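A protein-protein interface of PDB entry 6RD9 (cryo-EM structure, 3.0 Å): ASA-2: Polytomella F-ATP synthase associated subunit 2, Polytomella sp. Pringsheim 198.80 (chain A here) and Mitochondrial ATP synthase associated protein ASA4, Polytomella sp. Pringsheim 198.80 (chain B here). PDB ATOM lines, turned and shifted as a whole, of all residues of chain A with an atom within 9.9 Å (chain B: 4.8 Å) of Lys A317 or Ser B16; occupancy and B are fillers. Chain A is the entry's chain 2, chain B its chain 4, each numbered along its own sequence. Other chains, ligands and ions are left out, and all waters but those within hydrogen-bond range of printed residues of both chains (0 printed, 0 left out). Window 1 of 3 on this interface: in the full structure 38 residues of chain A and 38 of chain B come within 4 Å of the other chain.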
ATOM      1  N   GLU A 277      -9.342  18.861  26.779  1.00  0.00           N
ATOM      2  CA  GLU A 277     -10.001  18.811  25.494  1.00  0.00           C
ATOM      3  C   GLU A 277      -9.784  20.122  24.756  1.00  0.00           C
ATOM      4  O   GLU A 277      -9.561  21.172  25.354  1.00  0.00           O
ATOM      5  CB  GLU A 277     -11.496  18.575  25.669  1.00  0.00           C
ATOM      6  CG  GLU A 277     -11.872  17.216  26.196  1.00  0.00           C
ATOM      7  CD  GLU A 277     -11.675  16.123  25.178  1.00  0.00           C
ATOM      8  OE1 GLU A 277     -11.859  16.396  23.975  1.00  0.00           O
ATOM      9  OE2 GLU A 277     -11.337  14.989  25.574  1.00  0.00           O
ATOM     10  N   VAL A 278      -9.879  20.058  23.431  1.00  0.00           N
ATOM     11  CA  VAL A 278      -9.810  21.275  22.650  1.00  0.00           C
ATOM     12  C   VAL A 278     -11.104  22.067  22.789  1.00  0.00           C
ATOM     13  O   VAL A 278     -11.137  23.260  22.494  1.00  0.00           O
ATOM     14  CB  VAL A 278      -9.451  20.897  21.208  1.00  0.00           C
ATOM     15  CG1 VAL A 278      -9.042  22.085  20.403  1.00  0.00           C
ATOM     16  CG2 VAL A 278      -8.328  19.918  21.231  1.00  0.00           C
ATOM     17  N   SER A 279     -12.178  21.444  23.268  1.00  0.00           N
ATOM     18  CA  SER A 279     -13.349  22.222  23.643  1.00  0.00           C
ATOM     19  C   SER A 279     -13.104  22.992  24.924  1.00  0.00           C
ATOM     20  O   SER A 279     -13.727  24.028  25.148  1.00  0.00           O
ATOM     21  CB  SER A 279     -14.568  21.331  23.816  1.00  0.00           C
ATOM     22  OG  SER A 279     -14.461  20.579  25.005  1.00  0.00           O
ATOM     23  N   LEU A 309      -9.212  26.134  16.323  1.00  0.00           N
ATOM     24  CA  LEU A 309      -9.432  24.721  16.057  1.00  0.00           C
ATOM     25  C   LEU A 309     -10.834  24.303  16.450  1.00  0.00           C
ATOM     26  O   LEU A 309     -11.521  23.633  15.682  1.00  0.00           O
ATOM     27  CB  LEU A 309      -8.412  23.879  16.805  1.00  0.00           C
ATOM     28  CG  LEU A 309      -7.016  23.817  16.223  1.00  0.00           C
ATOM     29  CD1 LEU A 309      -6.192  22.903  17.049  1.00  0.00           C
ATOM     30  CD2 LEU A 309      -7.072  23.319  14.823  1.00  0.00           C
ATOM     31  N   ALA A 310     -11.290  24.697  17.627  1.00  0.00           N
ATOM     32  CA  ALA A 310     -12.582  24.220  18.078  1.00  0.00           C
ATOM     33  C   ALA A 310     -13.746  24.915  17.405  1.00  0.00           C
ATOM     34  O   ALA A 310     -14.888  24.515  17.631  1.00  0.00           O
ATOM     35  CB  ALA A 310     -12.710  24.378  19.582  1.00  0.00           C
ATOM     36  N   ALA A 311     -13.496  25.953  16.609  1.00  0.00           N
ATOM     37  CA  ALA A 311     -14.577  26.628  15.904  1.00  0.00           C
ATOM     38  C   ALA A 311     -14.768  26.066  14.509  1.00  0.00           C
ATOM     39  O   ALA A 311     -15.890  26.051  14.000  1.00  0.00           O
ATOM     40  CB  ALA A 311     -14.315  28.128  15.837  1.00  0.00           C
ATOM     41  N   ASP A 312     -13.692  25.623  13.865  1.00  0.00           N
ATOM     42  CA  ASP A 312     -13.863  24.916  12.608  1.00  0.00           C
ATOM     43  C   ASP A 312     -14.416  23.523  12.809  1.00  0.00           C
ATOM     44  O   ASP A 312     -15.169  23.040  11.964  1.00  0.00           O
ATOM     45  CB  ASP A 312     -12.554  24.803  11.854  1.00  0.00           C
ATOM     46  CG  ASP A 312     -11.869  26.098  11.716  1.00  0.00           C
ATOM     47  OD1 ASP A 312     -10.635  26.145  11.866  1.00  0.00           O
ATOM     48  OD2 ASP A 312     -12.579  27.084  11.468  1.00  0.00           O
ATOM     49  N   ALA A 313     -14.051  22.869  13.905  1.00  0.00           N
ATOM     50  CA  ALA A 313     -14.541  21.531  14.172  1.00  0.00           C
ATOM     51  C   ALA A 313     -16.037  21.520  14.395  1.00  0.00           C
ATOM     52  O   ALA A 313     -16.692  20.525  14.091  1.00  0.00           O
ATOM     53  CB  ALA A 313     -13.828  20.949  15.380  1.00  0.00           C
ATOM     54  N   ALA A 314     -16.596  22.598  14.917  1.00  0.00           N
ATOM     55  CA  ALA A 314     -18.040  22.697  14.999  1.00  0.00           C
ATOM     56  C   ALA A 314     -18.652  23.244  13.727  1.00  0.00           C
ATOM     57  O   ALA A 314     -19.875  23.203  13.583  1.00  0.00           O
ATOM     58  CB  ALA A 314     -18.443  23.567  16.181  1.00  0.00           C
ATOM     59  N   ARG A 315     -17.841  23.776  12.819  1.00  0.00           N
ATOM     60  CA  ARG A 315     -18.324  24.183  11.509  1.00  0.00           C
ATOM     61  C   ARG A 315     -18.269  23.051  10.501  1.00  0.00           C
ATOM     62  O   ARG A 315     -19.151  22.945   9.647  1.00  0.00           O
ATOM     63  CB  ARG A 315     -17.506  25.360  10.991  1.00  0.00           C
ATOM     64  CG  ARG A 315     -18.121  26.041   9.818  1.00  0.00           C
ATOM     65  CD  ARG A 315     -17.195  27.022   9.189  1.00  0.00           C
ATOM     66  NE  ARG A 315     -17.714  27.432   7.898  1.00  0.00           N
ATOM     67  CZ  ARG A 315     -17.374  26.865   6.752  1.00  0.00           C
ATOM     68  NH1 ARG A 315     -16.500  25.876   6.734  1.00  0.00           N
ATOM     69  NH2 ARG A 315     -17.901  27.295   5.619  1.00  0.00           N
ATOM     70  N   LEU A 316     -17.242  22.207  10.582  1.00  0.00           N
ATOM     71  CA  LEU A 316     -17.191  21.004   9.768  1.00  0.00           C
ATOM     72  C   LEU A 316     -18.296  20.032  10.128  1.00  0.00           C
ATOM     73  O   LEU A 316     -18.863  19.384   9.246  1.00  0.00           O
ATOM     74  CB  LEU A 316     -15.845  20.326   9.940  1.00  0.00           C
ATOM     75  CG  LEU A 316     -14.901  20.523   8.782  1.00  0.00           C
ATOM     76  CD1 LEU A 316     -13.577  19.946   9.136  1.00  0.00           C
ATOM     77  CD2 LEU A 316     -15.482  19.795   7.618  1.00  0.00           C
ATOM     78  N   LYS A 317     -18.623  19.922  11.405  1.00  0.00           N
ATOM     79  CA  LYS A 317     -19.660  19.013  11.870  1.00  0.00           C
ATOM     80  C   LYS A 317     -20.968  19.742  12.100  1.00  0.00           C
ATOM     81  O   LYS A 317     -21.696  19.444  13.043  1.00  0.00           O
ATOM     82  CB  LYS A 317     -19.199  18.306  13.132  1.00  0.00           C
ATOM     83  CG  LYS A 317     -17.864  17.610  12.977  1.00  0.00           C
ATOM     84  CD  LYS A 317     -17.613  16.704  14.142  1.00  0.00           C
ATOM     85  CE  LYS A 317     -16.274  16.040  14.044  1.00  0.00           C
ATOM     86  NZ  LYS A 317     -16.103  15.040  15.129  1.00  0.00           N
ATOM     87  N   ARG A 318     -21.262  20.714  11.242  1.00  0.00           N
ATOM     88  CA  ARG A 318     -22.439  21.559  11.365  1.00  0.00           C
ATOM     89  C   ARG A 318     -23.713  20.761  11.135  1.00  0.00           C
ATOM     90  O   ARG A 318     -23.744  19.814  10.352  1.00  0.00           O
ATOM     91  CB  ARG A 318     -22.348  22.706  10.364  1.00  0.00           C
ATOM     92  CG  ARG A 318     -23.304  23.838  10.595  1.00  0.00           C
ATOM     93  CD  ARG A 318     -23.026  25.004   9.698  1.00  0.00           C
ATOM     94  NE  ARG A 318     -22.348  26.061  10.414  1.00  0.00           N
ATOM     95  CZ  ARG A 318     -21.506  26.901   9.844  1.00  0.00           C
ATOM     96  NH1 ARG A 318     -21.240  26.780   8.554  1.00  0.00           N
ATOM     97  NH2 ARG A 318     -20.919  27.844  10.562  1.00  0.00           N
ATOM     98  N   SER A 319     -24.782  21.184  11.805  1.00  0.00           N
ATOM     99  CA  SER A 319     -26.006  20.411  11.956  1.00  0.00           C
ATOM    100  C   SER A 319     -26.815  20.217  10.685  1.00  0.00           C
ATOM    101  O   SER A 319     -27.880  19.604  10.770  1.00  0.00           O
ATOM    102  CB  SER A 319     -26.904  21.088  12.979  1.00  0.00           C
ATOM    103  OG  SER A 319     -28.197  20.520  12.955  1.00  0.00           O
ATOM    104  N   SER A 320     -26.431  20.823   9.559  1.00  0.00           N
ATOM    105  CA  SER A 320     -27.091  20.731   8.248  1.00  0.00           C
ATOM    106  C   SER A 320     -28.522  21.267   8.177  1.00  0.00           C
ATOM    107  O   SER A 320     -29.091  21.355   7.089  1.00  0.00           O
ATOM    108  CB  SER A 320     -27.091  19.302   7.714  1.00  0.00           C
ATOM    109  OG  SER A 320     -27.794  19.252   6.488  1.00  0.00           O
ATOM    110  N   ALA A 321     -29.122  21.600   9.313  1.00  0.00           N
ATOM    111  CA  ALA A 321     -30.171  22.589   9.411  1.00  0.00           C
ATOM    112  C   ALA A 321     -29.621  23.898   9.925  1.00  0.00           C
ATOM    113  O   ALA A 321     -30.335  24.898   9.934  1.00  0.00           O
ATOM    114  CB  ALA A 321     -31.290  22.105  10.329  1.00  0.00           C
ATOM    115  N   GLU A 322     -28.383  23.888  10.405  1.00  0.00           N
ATOM    116  CA  GLU A 322     -27.622  25.106  10.593  1.00  0.00           C
ATOM    117  C   GLU A 322     -26.925  25.508   9.309  1.00  0.00           C
ATOM    118  O   GLU A 322     -26.741  26.699   9.055  1.00  0.00           O
ATOM    119  CB  GLU A 322     -26.608  24.916  11.713  1.00  0.00           C
ATOM    120  CG  GLU A 322     -25.924  26.181  12.167  1.00  0.00           C
ATOM    121  CD  GLU A 322     -24.850  25.936  13.201  1.00  0.00           C
ATOM    122  OE1 GLU A 322     -23.659  26.141  12.893  1.00  0.00           O
ATOM    123  OE2 GLU A 322     -25.195  25.530  14.326  1.00  0.00           O
ATOM    124  N   SER A 323     -26.537  24.538   8.482  1.00  0.00           N
ATOM    125  CA  SER A 323     -25.985  24.868   7.174  1.00  0.00           C
ATOM    126  C   SER A 323     -27.051  25.413   6.242  1.00  0.00           C
ATOM    127  O   SER A 323     -26.729  26.139   5.300  1.00  0.00           O
ATOM    128  CB  SER A 323     -25.325  23.646   6.547  1.00  0.00           C
ATOM    129  OG  SER A 323     -24.026  23.436   7.057  1.00  0.00           O
ATOM    130  N   SER A 381     -30.355  24.964  18.440  1.00  0.00           N
ATOM    131  CA  SER A 381     -29.556  24.259  19.423  1.00  0.00           C
ATOM    132  C   SER A 381     -28.822  25.231  20.325  1.00  0.00           C
ATOM    133  O   SER A 381     -28.436  24.869  21.439  1.00  0.00           O
ATOM    134  CB  SER A 381     -28.579  23.329  18.713  1.00  0.00           C
ATOM    135  OG  SER A 381     -27.682  24.058  17.902  1.00  0.00           O
ATOM    136  N   LEU B  12      -9.420  18.189  12.571  1.00  0.00           N
ATOM    137  CA  LEU B  12     -10.637  18.853  13.010  1.00  0.00           C
ATOM    138  C   LEU B  12     -11.750  17.859  13.229  1.00  0.00           C
ATOM    139  O   LEU B  12     -12.676  18.123  13.996  1.00  0.00           O
ATOM    140  CB  LEU B  12     -11.085  19.878  11.984  1.00  0.00           C
ATOM    141  CG  LEU B  12     -10.225  21.114  11.850  1.00  0.00           C
ATOM    142  CD1 LEU B  12     -10.667  21.856  10.638  1.00  0.00           C
ATOM    143  CD2 LEU B  12     -10.378  21.969  13.062  1.00  0.00           C
ATOM    144  N   TYR B  13     -11.639  16.706  12.562  1.00  0.00           N
ATOM    145  CA  TYR B  13     -12.659  15.631  12.660  1.00  0.00           C
ATOM    146  C   TYR B  13     -12.294  14.657  13.787  1.00  0.00           C
ATOM    147  O   TYR B  13     -13.139  13.804  14.124  1.00  0.00           O
ATOM    148  CB  TYR B  13     -12.794  14.898  11.322  1.00  0.00           C
ATOM    149  CG  TYR B  13     -14.148  15.016  10.670  1.00  0.00           C
ATOM    150  CD1 TYR B  13     -15.151  14.098  10.935  1.00  0.00           C
ATOM    151  CD2 TYR B  13     -14.430  16.045   9.787  1.00  0.00           C
ATOM    152  CE1 TYR B  13     -16.398  14.198  10.341  1.00  0.00           C
ATOM    153  CE2 TYR B  13     -15.672  16.161   9.184  1.00  0.00           C
ATOM    154  CZ  TYR B  13     -16.660  15.234   9.462  1.00  0.00           C
ATOM    155  OH  TYR B  13     -17.886  15.340   8.872  1.00  0.00           O
ATOM    156  N   PHE B  14     -11.086  14.776  14.350  1.00  0.00           N
ATOM    157  CA  PHE B  14     -10.698  13.873  15.413  1.00  0.00           C
ATOM    158  C   PHE B  14     -10.692  14.552  16.769  1.00  0.00           C
ATOM    159  O   PHE B  14     -10.204  13.968  17.734  1.00  0.00           O
ATOM    160  CB  PHE B  14      -9.325  13.264  15.132  1.00  0.00           C
ATOM    161  CG  PHE B  14      -9.238  12.471  13.855  1.00  0.00           C
ATOM    162  CD1 PHE B  14     -10.360  11.950  13.231  1.00  0.00           C
ATOM    163  CD2 PHE B  14      -8.008  12.219  13.296  1.00  0.00           C
ATOM    164  CE1 PHE B  14     -10.252  11.240  12.065  1.00  0.00           C
ATOM    165  CE2 PHE B  14      -7.902  11.494  12.133  1.00  0.00           C
ATOM    166  CZ  PHE B  14      -9.027  11.008  11.521  1.00  0.00           C
ATOM    167  N   LEU B  15     -11.201  15.777  16.861  1.00  0.00           N
ATOM    168  CA  LEU B  15     -11.229  16.471  18.142  1.00  0.00           C
ATOM    169  C   LEU B  15     -12.288  15.884  19.055  1.00  0.00           C
ATOM    170  O   LEU B  15     -12.025  15.602  20.227  1.00  0.00           O
ATOM    171  CB  LEU B  15     -11.487  17.959  17.938  1.00  0.00           C
ATOM    172  CG  LEU B  15     -10.425  18.825  17.285  1.00  0.00           C
ATOM    173  CD1 LEU B  15     -10.777  20.264  17.503  1.00  0.00           C
ATOM    174  CD2 LEU B  15      -9.059  18.517  17.831  1.00  0.00           C
ATOM    175  N   SER B  16     -13.502  15.721  18.551  1.00  0.00           N
ATOM    176  CA  SER B  16     -14.554  15.087  19.326  1.00  0.00           C
ATOM    177  C   SER B  16     -14.516  13.570  19.237  1.00  0.00           C
ATOM    178  O   SER B  16     -15.263  12.911  19.962  1.00  0.00           O
ATOM    179  CB  SER B  16     -15.928  15.589  18.881  1.00  0.00           C
ATOM    180  OG  SER B  16     -16.955  14.964  19.628  1.00  0.00           O
ATOM    181  N   SER B  17     -13.680  13.008  18.372  1.00  0.00           N
ATOM    182  CA  SER B  17     -13.441  11.577  18.375  1.00  0.00           C
ATOM    183  C   SER B  17     -12.732  11.145  19.650  1.00  0.00           C
ATOM    184  O   SER B  17     -12.020  11.916  20.297  1.00  0.00           O
ATOM    185  CB  SER B  17     -12.595  11.162  17.180  1.00  0.00           C
ATOM    186  OG  SER B  17     -12.209   9.808  17.305  1.00  0.00           O
ATOM    187  N   LYS B  18     -12.934   9.879  20.007  1.00  0.00           N
ATOM    188  CA  LYS B  18     -12.438   9.365  21.272  1.00  0.00           C
ATOM    189  C   LYS B  18     -11.743   8.016  21.150  1.00  0.00           C
ATOM    190  O   LYS B  18     -11.552   7.348  22.168  1.00  0.00           O
ATOM    191  CB  LYS B  18     -13.576   9.270  22.288  1.00  0.00           C
ATOM    192  CG  LYS B  18     -13.965  10.611  22.879  1.00  0.00           C
ATOM    193  CD  LYS B  18     -15.069  10.482  23.909  1.00  0.00           C
ATOM    194  CE  LYS B  18     -15.349  11.818  24.568  1.00  0.00           C
ATOM    195  NZ  LYS B  18     -14.172  12.327  25.320  1.00  0.00           N
ATOM    196  N   GLN B  95     -19.952  11.500  17.143  1.00  0.00           N
ATOM    197  CA  GLN B  95     -18.530  11.811  17.132  1.00  0.00           C
ATOM    198  C   GLN B  95     -18.000  11.943  15.723  1.00  0.00           C
ATOM    199  O   GLN B  95     -17.017  12.650  15.498  1.00  0.00           O
ATOM    200  CB  GLN B  95     -17.741  10.740  17.866  1.00  0.00           C
ATOM    201  CG  GLN B  95     -17.743  10.874  19.353  1.00  0.00           C
ATOM    202  CD  GLN B  95     -17.468   9.558  20.039  1.00  0.00           C
ATOM    203  OE1 GLN B  95     -16.714   8.726  19.534  1.00  0.00           O
ATOM    204  NE2 GLN B  95     -18.096   9.350  21.187  1.00  0.00           N
ATOM    205  N   ALA B  96     -18.626  11.277  14.770  1.00  0.00           N
ATOM    206  CA  ALA B  96     -18.183  11.288  13.390  1.00  0.00           C
ATOM    207  C   ALA B  96     -18.888  12.328  12.551  1.00  0.00           C
ATOM    208  O   ALA B  96     -18.675  12.368  11.344  1.00  0.00           O
ATOM    209  CB  ALA B  96     -18.394   9.925  12.762  1.00  0.00           C
ATOM    210  N   GLY B  97     -19.750  13.134  13.136  1.00  0.00           N
ATOM    211  CA  GLY B  97     -20.383  14.193  12.403  1.00  0.00           C
ATOM    212  C   GLY B  97     -21.766  13.895  11.900  1.00  0.00           C
ATOM    213  O   GLY B  97     -22.311  14.702  11.147  1.00  0.00           O
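NZ of Lys A317 lies within hydrogen-bond range of O of Tyr B13, 3.4 Å away. The side-chain amino group of Lys B18 is in salt-bridge range of the side-chain carboxylate of Glu A277, at 3.9 Å. The backbone carbonyl oxygen (O) of Gln B95 is in hydrogen-bond range of the side-chain amino group (NZ) of Lys A317 (2.6 Å).
Hydrophobic or aromatic side chains of chain B within 4 Å of the printed part of chain A: Leu B12, Tyr B13 and Leu B15. Among the printed residues, 13 pairs touch across the chains.
Tyr B13 touches two residues of chain A. Leu B15 touches just these residues of chain A: Glu A277, Val A278, Leu A309 and Ala A313. No residue of chain A comes within 4 Å of Ser B17. Gln B95 touches one residue of chain A. Printed residues of chain B within 4 Å of Asp A312: Leu B12 (3.7 Å). Of the printed residues of chain B, Val A278 touches Leu B15 (3.7 Å). Ser A279 touches none of the printed residues of chain B. Phe B14 touches none of the printed residues of chain A. The nearest residue of chain B that does not touch Lys A317 is Gly B97 (4.1 Å).
Among the printed residues, pairs that only touch across the chains: Leu A309 with Leu B12, Ala A313 with Leu B12, Asp A312 with Leu B12, Val A278 with Leu B15, Ala A313 with Leu B15, Leu A316 with Leu B12, Lys A317 with Ser B16, Glu A277 with Leu B15, Leu A309 with Leu B15 and Leu A316 with Tyr B13.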
